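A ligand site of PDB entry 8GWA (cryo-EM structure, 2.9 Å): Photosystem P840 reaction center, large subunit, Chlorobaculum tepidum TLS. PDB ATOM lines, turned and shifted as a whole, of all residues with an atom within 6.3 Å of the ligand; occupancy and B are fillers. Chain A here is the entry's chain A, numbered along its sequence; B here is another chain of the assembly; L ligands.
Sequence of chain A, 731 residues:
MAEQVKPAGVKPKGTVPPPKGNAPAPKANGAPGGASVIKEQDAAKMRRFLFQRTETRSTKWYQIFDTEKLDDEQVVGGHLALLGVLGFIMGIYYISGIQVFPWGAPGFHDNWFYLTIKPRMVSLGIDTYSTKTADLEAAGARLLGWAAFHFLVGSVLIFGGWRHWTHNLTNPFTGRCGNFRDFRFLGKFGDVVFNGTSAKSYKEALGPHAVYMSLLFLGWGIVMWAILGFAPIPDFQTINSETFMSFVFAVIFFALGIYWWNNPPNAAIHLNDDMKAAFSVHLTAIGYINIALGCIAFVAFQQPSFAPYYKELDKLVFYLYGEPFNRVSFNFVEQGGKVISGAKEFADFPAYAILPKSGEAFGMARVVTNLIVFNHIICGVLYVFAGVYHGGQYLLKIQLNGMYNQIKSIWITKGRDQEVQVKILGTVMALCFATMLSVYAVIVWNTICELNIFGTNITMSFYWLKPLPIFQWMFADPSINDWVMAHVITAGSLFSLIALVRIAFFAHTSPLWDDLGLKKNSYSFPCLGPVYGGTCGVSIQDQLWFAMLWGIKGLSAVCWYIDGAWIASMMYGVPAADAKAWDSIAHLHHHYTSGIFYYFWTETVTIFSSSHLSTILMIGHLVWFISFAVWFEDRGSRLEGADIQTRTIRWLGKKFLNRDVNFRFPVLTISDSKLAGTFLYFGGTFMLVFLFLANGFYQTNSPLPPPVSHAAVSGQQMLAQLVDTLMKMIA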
ATOM      1  N   PRO A 526      19.595 -16.844 -16.502  1.00  0.00           N
ATOM      2  CA  PRO A 526      19.777 -17.725 -17.654  1.00  0.00           C
ATOM      3  C   PRO A 526      20.003 -19.176 -17.286  1.00  0.00           C
ATOM      4  O   PRO A 526      19.816 -20.051 -18.146  1.00  0.00           O
ATOM      5  CB  PRO A 526      21.007 -17.144 -18.352  1.00  0.00           C
ATOM      6  CG  PRO A 526      21.802 -16.543 -17.235  1.00  0.00           C
ATOM      7  CD  PRO A 526      20.844 -16.142 -16.149  1.00  0.00           C
ATOM      8  N   CYS A 527      20.390 -19.460 -16.046  1.00  0.00           N
ATOM      9  CA  CYS A 527      20.874 -20.782 -15.689  1.00  0.00           C
ATOM     10  C   CYS A 527      21.078 -20.855 -14.190  1.00  0.00           C
ATOM     11  O   CYS A 527      21.065 -19.841 -13.489  1.00  0.00           O
ATOM     12  CB  CYS A 527      22.180 -21.104 -16.404  1.00  0.00           C
ATOM     13  SG  CYS A 527      23.449 -19.861 -16.057  1.00  0.00           S
ATOM     14  N   LEU A 528      21.268 -22.082 -13.709  1.00  0.00           N
ATOM     15  CA  LEU A 528      21.861 -22.327 -12.402  1.00  0.00           C
ATOM     16  C   LEU A 528      23.219 -22.994 -12.502  1.00  0.00           C
ATOM     17  O   LEU A 528      23.902 -23.154 -11.484  1.00  0.00           O
ATOM     18  CB  LEU A 528      20.945 -23.205 -11.542  1.00  0.00           C
ATOM     19  CG  LEU A 528      19.524 -22.710 -11.338  1.00  0.00           C
ATOM     20  CD1 LEU A 528      18.838 -23.621 -10.340  1.00  0.00           C
ATOM     21  CD2 LEU A 528      19.500 -21.264 -10.875  1.00  0.00           C
ATOM     22  N   GLY A 529      23.639 -23.399 -13.700  1.00  0.00           N
ATOM     23  CA  GLY A 529      24.939 -23.958 -13.899  1.00  0.00           C
ATOM     24  C   GLY A 529      24.928 -25.318 -14.569  1.00  0.00           C
ATOM     25  O   GLY A 529      23.889 -25.805 -15.013  1.00  0.00           O
ATOM     26  N   PRO A 530      26.111 -25.932 -14.657  1.00  0.00           N
ATOM     27  CA  PRO A 530      26.204 -27.280 -15.243  1.00  0.00           C
ATOM     28  C   PRO A 530      25.673 -28.375 -14.343  1.00  0.00           C
ATOM     29  O   PRO A 530      25.747 -29.553 -14.734  1.00  0.00           O
ATOM     30  CB  PRO A 530      27.714 -27.435 -15.477  1.00  0.00           C
ATOM     31  CG  PRO A 530      28.324 -26.570 -14.438  1.00  0.00           C
ATOM     32  CD  PRO A 530      27.421 -25.400 -14.265  1.00  0.00           C
ATOM     33  N   GLY A 534      23.482 -29.371 -16.661  1.00  0.00           N
ATOM     34  CA  GLY A 534      23.215 -28.066 -17.236  1.00  0.00           C
ATOM     35  C   GLY A 534      21.794 -27.587 -17.058  1.00  0.00           C
ATOM     36  O   GLY A 534      20.841 -28.358 -17.197  1.00  0.00           O
ATOM     37  N   THR A 535      21.641 -26.291 -16.744  1.00  0.00           N
ATOM     38  CA  THR A 535      20.342 -25.690 -16.462  1.00  0.00           C
ATOM     39  C   THR A 535      20.157 -24.419 -17.276  1.00  0.00           C
ATOM     40  O   THR A 535      19.627 -23.408 -16.803  1.00  0.00           O
ATOM     41  CB  THR A 535      20.205 -25.393 -14.966  1.00  0.00           C
ATOM     42  OG1 THR A 535      21.402 -24.753 -14.501  1.00  0.00           O
ATOM     43  CG2 THR A 535      19.998 -26.680 -14.190  1.00  0.00           C
ATOM     44  N   CYS A 536      20.574 -24.457 -18.546  1.00  0.00           N
ATOM     45  CA  CYS A 536      20.530 -23.271 -19.393  1.00  0.00           C
ATOM     46  C   CYS A 536      19.103 -22.931 -19.800  1.00  0.00           C
ATOM     47  O   CYS A 536      18.307 -23.813 -20.133  1.00  0.00           O
ATOM     48  CB  CYS A 536      21.363 -23.491 -20.653  1.00  0.00           C
ATOM     49  SG  CYS A 536      22.926 -24.327 -20.427  1.00  0.00           S
ATOM     50  N   GLY A 537      18.791 -21.636 -19.796  1.00  0.00           N
ATOM     51  CA  GLY A 537      17.586 -21.139 -20.428  1.00  0.00           C
ATOM     52  C   GLY A 537      16.271 -21.686 -19.920  1.00  0.00           C
ATOM     53  O   GLY A 537      15.410 -22.079 -20.718  1.00  0.00           O
ATOM     54  N   GLU A 633      27.253 -21.185 -25.998  1.00  0.00           N
ATOM     55  CA  GLU A 633      27.548 -21.201 -24.567  1.00  0.00           C
ATOM     56  C   GLU A 633      29.012 -20.790 -24.401  1.00  0.00           C
ATOM     57  O   GLU A 633      29.905 -21.601 -24.160  1.00  0.00           O
ATOM     58  CB  GLU A 633      27.253 -22.569 -23.969  1.00  0.00           C
ATOM     59  CG  GLU A 633      25.769 -22.929 -24.006  1.00  0.00           C
ATOM     60  CD  GLU A 633      25.524 -24.403 -24.241  1.00  0.00           C
ATOM     61  OE1 GLU A 633      26.461 -25.101 -24.665  1.00  0.00           O
ATOM     62  OE2 GLU A 633      24.399 -24.864 -23.995  1.00  0.00           O
ATOM     63  N   ASP A 634      29.246 -19.487 -24.536  1.00  0.00           N
ATOM     64  CA  ASP A 634      30.600 -18.954 -24.629  1.00  0.00           C
ATOM     65  C   ASP A 634      30.806 -17.693 -23.805  1.00  0.00           C
ATOM     66  O   ASP A 634      31.852 -17.040 -23.970  1.00  0.00           O
ATOM     67  CB  ASP A 634      30.955 -18.675 -26.092  1.00  0.00           C
ATOM     68  CG  ASP A 634      30.120 -17.554 -26.698  1.00  0.00           C
ATOM     69  OD1 ASP A 634      30.310 -16.387 -26.311  1.00  0.00           O
ATOM     70  OD2 ASP A 634      29.301 -17.841 -27.585  1.00  0.00           O
ATOM     71  N   ARG A 635      29.866 -17.321 -22.934  1.00  0.00           N
ATOM     72  CA  ARG A 635      29.971 -16.047 -22.240  1.00  0.00           C
ATOM     73  C   ARG A 635      31.209 -15.983 -21.361  1.00  0.00           C
ATOM     74  O   ARG A 635      31.863 -14.935 -21.275  1.00  0.00           O
ATOM     75  CB  ARG A 635      28.713 -15.790 -21.403  1.00  0.00           C
ATOM     76  CG  ARG A 635      28.543 -14.341 -21.022  1.00  0.00           C
ATOM     77  CD  ARG A 635      29.106 -14.069 -19.645  1.00  0.00           C
ATOM     78  NE  ARG A 635      29.259 -12.645 -19.374  1.00  0.00           N
ATOM     79  CZ  ARG A 635      29.821 -12.146 -18.280  1.00  0.00           C
ATOM     80  NH1 ARG A 635      30.322 -12.923 -17.343  1.00  0.00           N
ATOM     81  NH2 ARG A 635      29.898 -10.828 -18.142  1.00  0.00           N
ATOM     82  N   ILE A 670      24.789 -13.625 -19.785  1.00  0.00           N
ATOM     83  CA  ILE A 670      23.948 -14.528 -20.570  1.00  0.00           C
ATOM     84  C   ILE A 670      22.506 -14.031 -20.590  1.00  0.00           C
ATOM     85  O   ILE A 670      21.763 -14.320 -21.527  1.00  0.00           O
ATOM     86  CB  ILE A 670      24.054 -15.972 -20.056  1.00  0.00           C
ATOM     87  CG1 ILE A 670      25.492 -16.456 -20.076  1.00  0.00           C
ATOM     88  CG2 ILE A 670      23.273 -16.911 -20.965  1.00  0.00           C
ATOM     89  CD1 ILE A 670      26.160 -16.358 -18.757  1.00  0.00           C
ATOM     90  N   LYS A 674      21.493 -13.273 -24.133  1.00  0.00           N
ATOM     91  CA  LYS A 674      20.311 -13.854 -24.743  1.00  0.00           C
ATOM     92  C   LYS A 674      19.357 -12.782 -25.270  1.00  0.00           C
ATOM     93  O   LYS A 674      18.772 -12.947 -26.347  1.00  0.00           O
ATOM     94  CB  LYS A 674      19.575 -14.762 -23.763  1.00  0.00           C
ATOM     95  CG  LYS A 674      20.246 -16.109 -23.536  1.00  0.00           C
ATOM     96  CD  LYS A 674      19.756 -16.719 -22.232  1.00  0.00           C
ATOM     97  CE  LYS A 674      20.032 -18.198 -22.183  1.00  0.00           C
ATOM     98  NZ  LYS A 674      18.850 -18.984 -22.621  1.00  0.00           N
ATOM     99  N   PRO B 526      31.746 -27.279 -18.941  1.00  0.00           N
ATOM    100  CA  PRO B 526      31.284 -26.183 -19.791  1.00  0.00           C
ATOM    101  C   PRO B 526      31.357 -24.817 -19.136  1.00  0.00           C
ATOM    102  O   PRO B 526      31.538 -23.809 -19.830  1.00  0.00           O
ATOM    103  CB  PRO B 526      29.832 -26.565 -20.075  1.00  0.00           C
ATOM    104  CG  PRO B 526      29.407 -27.326 -18.871  1.00  0.00           C
ATOM    105  CD  PRO B 526      30.639 -27.965 -18.263  1.00  0.00           C
ATOM    106  N   CYS B 527      31.247 -24.760 -17.814  1.00  0.00           N
ATOM    107  CA  CYS B 527      31.003 -23.488 -17.127  1.00  0.00           C
ATOM    108  C   CYS B 527      31.017 -23.730 -15.619  1.00  0.00           C
ATOM    109  O   CYS B 527      31.184 -24.860 -15.150  1.00  0.00           O
ATOM    110  CB  CYS B 527      29.665 -22.889 -17.563  1.00  0.00           C
ATOM    111  SG  CYS B 527      28.299 -24.039 -17.308  1.00  0.00           S
ATOM    112  N   LEU B 528      30.844 -22.651 -14.874  1.00  0.00           N
ATOM    113  CA  LEU B 528      30.628 -22.684 -13.430  1.00  0.00           C
ATOM    114  C   LEU B 528      29.349 -21.944 -13.070  1.00  0.00           C
ATOM    115  O   LEU B 528      29.239 -21.343 -12.002  1.00  0.00           O
ATOM    116  CB  LEU B 528      31.811 -22.097 -12.676  1.00  0.00           C
ATOM    117  CG  LEU B 528      33.147 -22.799 -12.837  1.00  0.00           C
ATOM    118  CD1 LEU B 528      34.243 -21.934 -12.277  1.00  0.00           C
ATOM    119  CD2 LEU B 528      33.118 -24.147 -12.168  1.00  0.00           C
ATOM    120  N   GLY B 529      28.370 -21.973 -13.967  1.00  0.00           N
ATOM    121  CA  GLY B 529      27.078 -21.376 -13.690  1.00  0.00           C
ATOM    122  C   GLY B 529      27.010 -19.891 -13.975  1.00  0.00           C
ATOM    123  O   GLY B 529      27.909 -19.297 -14.584  1.00  0.00           O
ATOM    124  N   PRO B 530      25.924 -19.260 -13.520  1.00  0.00           N
ATOM    125  CA  PRO B 530      25.728 -17.824 -13.739  1.00  0.00           C
ATOM    126  C   PRO B 530      26.562 -16.921 -12.839  1.00  0.00           C
ATOM    127  O   PRO B 530      26.289 -15.718 -12.783  1.00  0.00           O
ATOM    128  CB  PRO B 530      24.235 -17.647 -13.440  1.00  0.00           C
ATOM    129  CG  PRO B 530      23.932 -18.696 -12.446  1.00  0.00           C
ATOM    130  CD  PRO B 530      24.805 -19.874 -12.785  1.00  0.00           C
ATOM    131  N   GLY B 534      28.535 -15.122 -15.533  1.00  0.00           N
ATOM    132  CA  GLY B 534      28.646 -16.240 -16.440  1.00  0.00           C
ATOM    133  C   GLY B 534      30.058 -16.723 -16.671  1.00  0.00           C
ATOM    134  O   GLY B 534      30.999 -15.934 -16.718  1.00  0.00           O
ATOM    135  N   THR B 535      30.223 -18.043 -16.815  1.00  0.00           N
ATOM    136  CA  THR B 535      31.515 -18.671 -17.016  1.00  0.00           C
ATOM    137  C   THR B 535      31.436 -19.711 -18.129  1.00  0.00           C
ATOM    138  O   THR B 535      32.090 -20.751 -18.082  1.00  0.00           O
ATOM    139  CB  THR B 535      32.015 -19.306 -15.718  1.00  0.00           C
ATOM    140  OG1 THR B 535      30.933 -19.983 -15.073  1.00  0.00           O
ATOM    141  CG2 THR B 535      32.566 -18.245 -14.787  1.00  0.00           C
ATOM    142  N   CYS B 536      30.634 -19.423 -19.148  1.00  0.00           N
ATOM    143  CA  CYS B 536      30.380 -20.382 -20.215  1.00  0.00           C
ATOM    144  C   CYS B 536      31.621 -20.628 -21.066  1.00  0.00           C
ATOM    145  O   CYS B 536      32.357 -19.701 -21.387  1.00  0.00           O
ATOM    146  CB  CYS B 536      29.252 -19.878 -21.117  1.00  0.00           C
ATOM    147  SG  CYS B 536      27.755 -19.341 -20.265  1.00  0.00           S
ATOM    148  N   GLY B 537      31.833 -21.894 -21.427  1.00  0.00           N
ATOM    149  CA  GLY B 537      32.812 -22.239 -22.435  1.00  0.00           C
ATOM    150  C   GLY B 537      34.250 -21.864 -22.166  1.00  0.00           C
ATOM    151  O   GLY B 537      34.927 -21.337 -23.050  1.00  0.00           O
ATOM    152  N   GLU B 633      22.324 -21.404 -25.352  1.00  0.00           N
ATOM    153  CA  GLU B 633      22.232 -21.617 -23.910  1.00  0.00           C
ATOM    154  C   GLU B 633      20.811 -22.094 -23.639  1.00  0.00           C
ATOM    155  O   GLU B 633      19.924 -21.338 -23.240  1.00  0.00           O
ATOM    156  CB  GLU B 633      22.559 -20.368 -23.098  1.00  0.00           C
ATOM    157  CG  GLU B 633      24.018 -19.965 -23.038  1.00  0.00           C
ATOM    158  CD  GLU B 633      24.306 -18.695 -23.799  1.00  0.00           C
ATOM    159  OE1 GLU B 633      23.584 -18.395 -24.769  1.00  0.00           O
ATOM    160  OE2 GLU B 633      25.269 -17.979 -23.437  1.00  0.00           O
ATOM    161  N   ASP B 634      20.585 -23.392 -23.881  1.00  0.00           N
ATOM    162  CA  ASP B 634      19.240 -23.942 -23.777  1.00  0.00           C
ATOM    163  C   ASP B 634      19.197 -25.335 -23.166  1.00  0.00           C
ATOM    164  O   ASP B 634      18.145 -25.969 -23.201  1.00  0.00           O
ATOM    165  CB  ASP B 634      18.575 -23.957 -25.159  1.00  0.00           C
ATOM    166  CG  ASP B 634      19.269 -24.892 -26.138  1.00  0.00           C
ATOM    167  OD1 ASP B 634      20.365 -25.403 -25.832  1.00  0.00           O
ATOM    168  OD2 ASP B 634      18.703 -25.118 -27.226  1.00  0.00           O
ATOM    169  N   ARG B 635      20.312 -25.820 -22.603  1.00  0.00           N
ATOM    170  CA  ARG B 635      20.367 -27.198 -22.132  1.00  0.00           C
ATOM    171  C   ARG B 635      19.335 -27.459 -21.038  1.00  0.00           C
ATOM    172  O   ARG B 635      18.679 -28.500 -21.029  1.00  0.00           O
ATOM    173  CB  ARG B 635      21.763 -27.534 -21.629  1.00  0.00           C
ATOM    174  CG  ARG B 635      22.066 -29.016 -21.598  1.00  0.00           C
ATOM    175  CD  ARG B 635      21.742 -29.612 -20.242  1.00  0.00           C
ATOM    176  NE  ARG B 635      21.705 -31.065 -20.260  1.00  0.00           N
ATOM    177  CZ  ARG B 635      21.422 -31.831 -19.215  1.00  0.00           C
ATOM    178  NH1 ARG B 635      21.125 -31.303 -18.041  1.00  0.00           N
ATOM    179  NH2 ARG B 635      21.437 -33.152 -19.354  1.00  0.00           N
ATOM    180  N   ILE B 670      25.827 -30.249 -21.132  1.00  0.00           N
ATOM    181  CA  ILE B 670      26.356 -29.092 -21.845  1.00  0.00           C
ATOM    182  C   ILE B 670      27.666 -29.455 -22.553  1.00  0.00           C
ATOM    183  O   ILE B 670      27.943 -28.955 -23.648  1.00  0.00           O
ATOM    184  CB  ILE B 670      26.560 -27.900 -20.910  1.00  0.00           C
ATOM    185  CG1 ILE B 670      25.324 -27.641 -20.062  1.00  0.00           C
ATOM    186  CG2 ILE B 670      26.789 -26.644 -21.725  1.00  0.00           C
ATOM    187  CD1 ILE B 670      25.435 -26.365 -19.253  1.00  0.00           C
ATOM    188  N   LYS B 674      27.753 -29.284 -26.468  1.00  0.00           N
ATOM    189  CA  LYS B 674      28.727 -28.503 -27.222  1.00  0.00           C
ATOM    190  C   LYS B 674      29.507 -29.372 -28.199  1.00  0.00           C
ATOM    191  O   LYS B 674      29.776 -28.952 -29.329  1.00  0.00           O
ATOM    192  CB  LYS B 674      29.689 -27.794 -26.258  1.00  0.00           C
ATOM    193  CG  LYS B 674      29.052 -26.672 -25.472  1.00  0.00           C
ATOM    194  CD  LYS B 674      30.087 -26.029 -24.581  1.00  0.00           C
ATOM    195  CE  LYS B 674      29.464 -25.185 -23.503  1.00  0.00           C
ATOM    196  NZ  LYS B 674      30.480 -24.368 -22.780  1.00  0.00           N
HETATM  197 FE1  LIG L   1      26.152 -20.805 -19.687  1.00  0.00          FE
HETATM  198 FE2  LIG L   1      24.324 -22.754 -19.630  1.00  0.00          FE
HETATM  199 FE3  LIG L   1      24.613 -21.135 -17.481  1.00  0.00          FE
HETATM  200 FE4  LIG L   1      26.490 -22.925 -18.061  1.00  0.00          FE
HETATM  201  S1  LIG L   1      24.369 -23.397 -17.458  1.00  0.00           S
HETATM  202  S2  LIG L   1      26.830 -20.747 -17.503  1.00  0.00           S
HETATM  203  S3  LIG L   1      26.467 -22.982 -20.353  1.00  0.00           S
HETATM  204  S4  LIG L   1      23.919 -20.507 -19.582  1.00  0.00           S
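O of Gly 529 of chain A sits close to S1 of the ligand.
S2 of the ligand lies close to O of Gly 529 of chain B (3.4 Å).
Merely in contact with the ligand: Glu 633 of chain B (3.5 Å), Ile 670 of chain B (3.6 Å), Glu 633 of chain A (3.7 Å) and Ile 670 of chain A (3.9 Å).
Hydrophobic or aromatic side chains that line the ligand: Ile 670 of chain A and Ile 670 of chain B.
Of the 28 residues printed, 10 come within 4 Å of the ligand.
Along chain A the residues within 4 Å of the ligand span positions 527 to 670.
The nearest printed residue that does not touch the ligand is Thr 535 of chain A (4.04 Å).
The side-chain sulfur (SG) of Cys 527 of chain B is bound to an iron atom (FE4) of the ligand (2.3 Å).
SG of Cys 527 of chain A binds FE3 of the ligand.
SG of Cys 536 of chain A is bound to FE2 of the ligand (2.3 Å).
SG of Cys 536 of chain B is bound to FE1 of the ligand (2.2 Å).
The backbone carbonyl oxygen of Glu 633 of chain A is in hydrogen-bond range of the side-chain amino group of Lys 674 of chain B (3.1 Å).
N of Arg 635 of chain B sits close to SG of Cys 536 of chain A (3.7 Å).
The backbone carbonyl oxygen (O) of Glu 633 of chain B sits at hydrogen-bond distance from the side-chain amino group (NZ) of Lys 674 of chain A, 2.7 Å away.
The backbone carbonyl oxygen (O) of Gly 529 of chain B lies within hydrogen-bond range of the side-chain hydroxyl (OG1) of Thr 535 of chain B, 3.1 Å away.
OG1 of Thr 535 of chain A sits at hydrogen-bond distance from N of Gly 529 of chain A (2.7 Å).
O of Glu 633 of chain A is in hydrogen-bond range of N of Gly 537 of chain B, 3.4 Å away.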
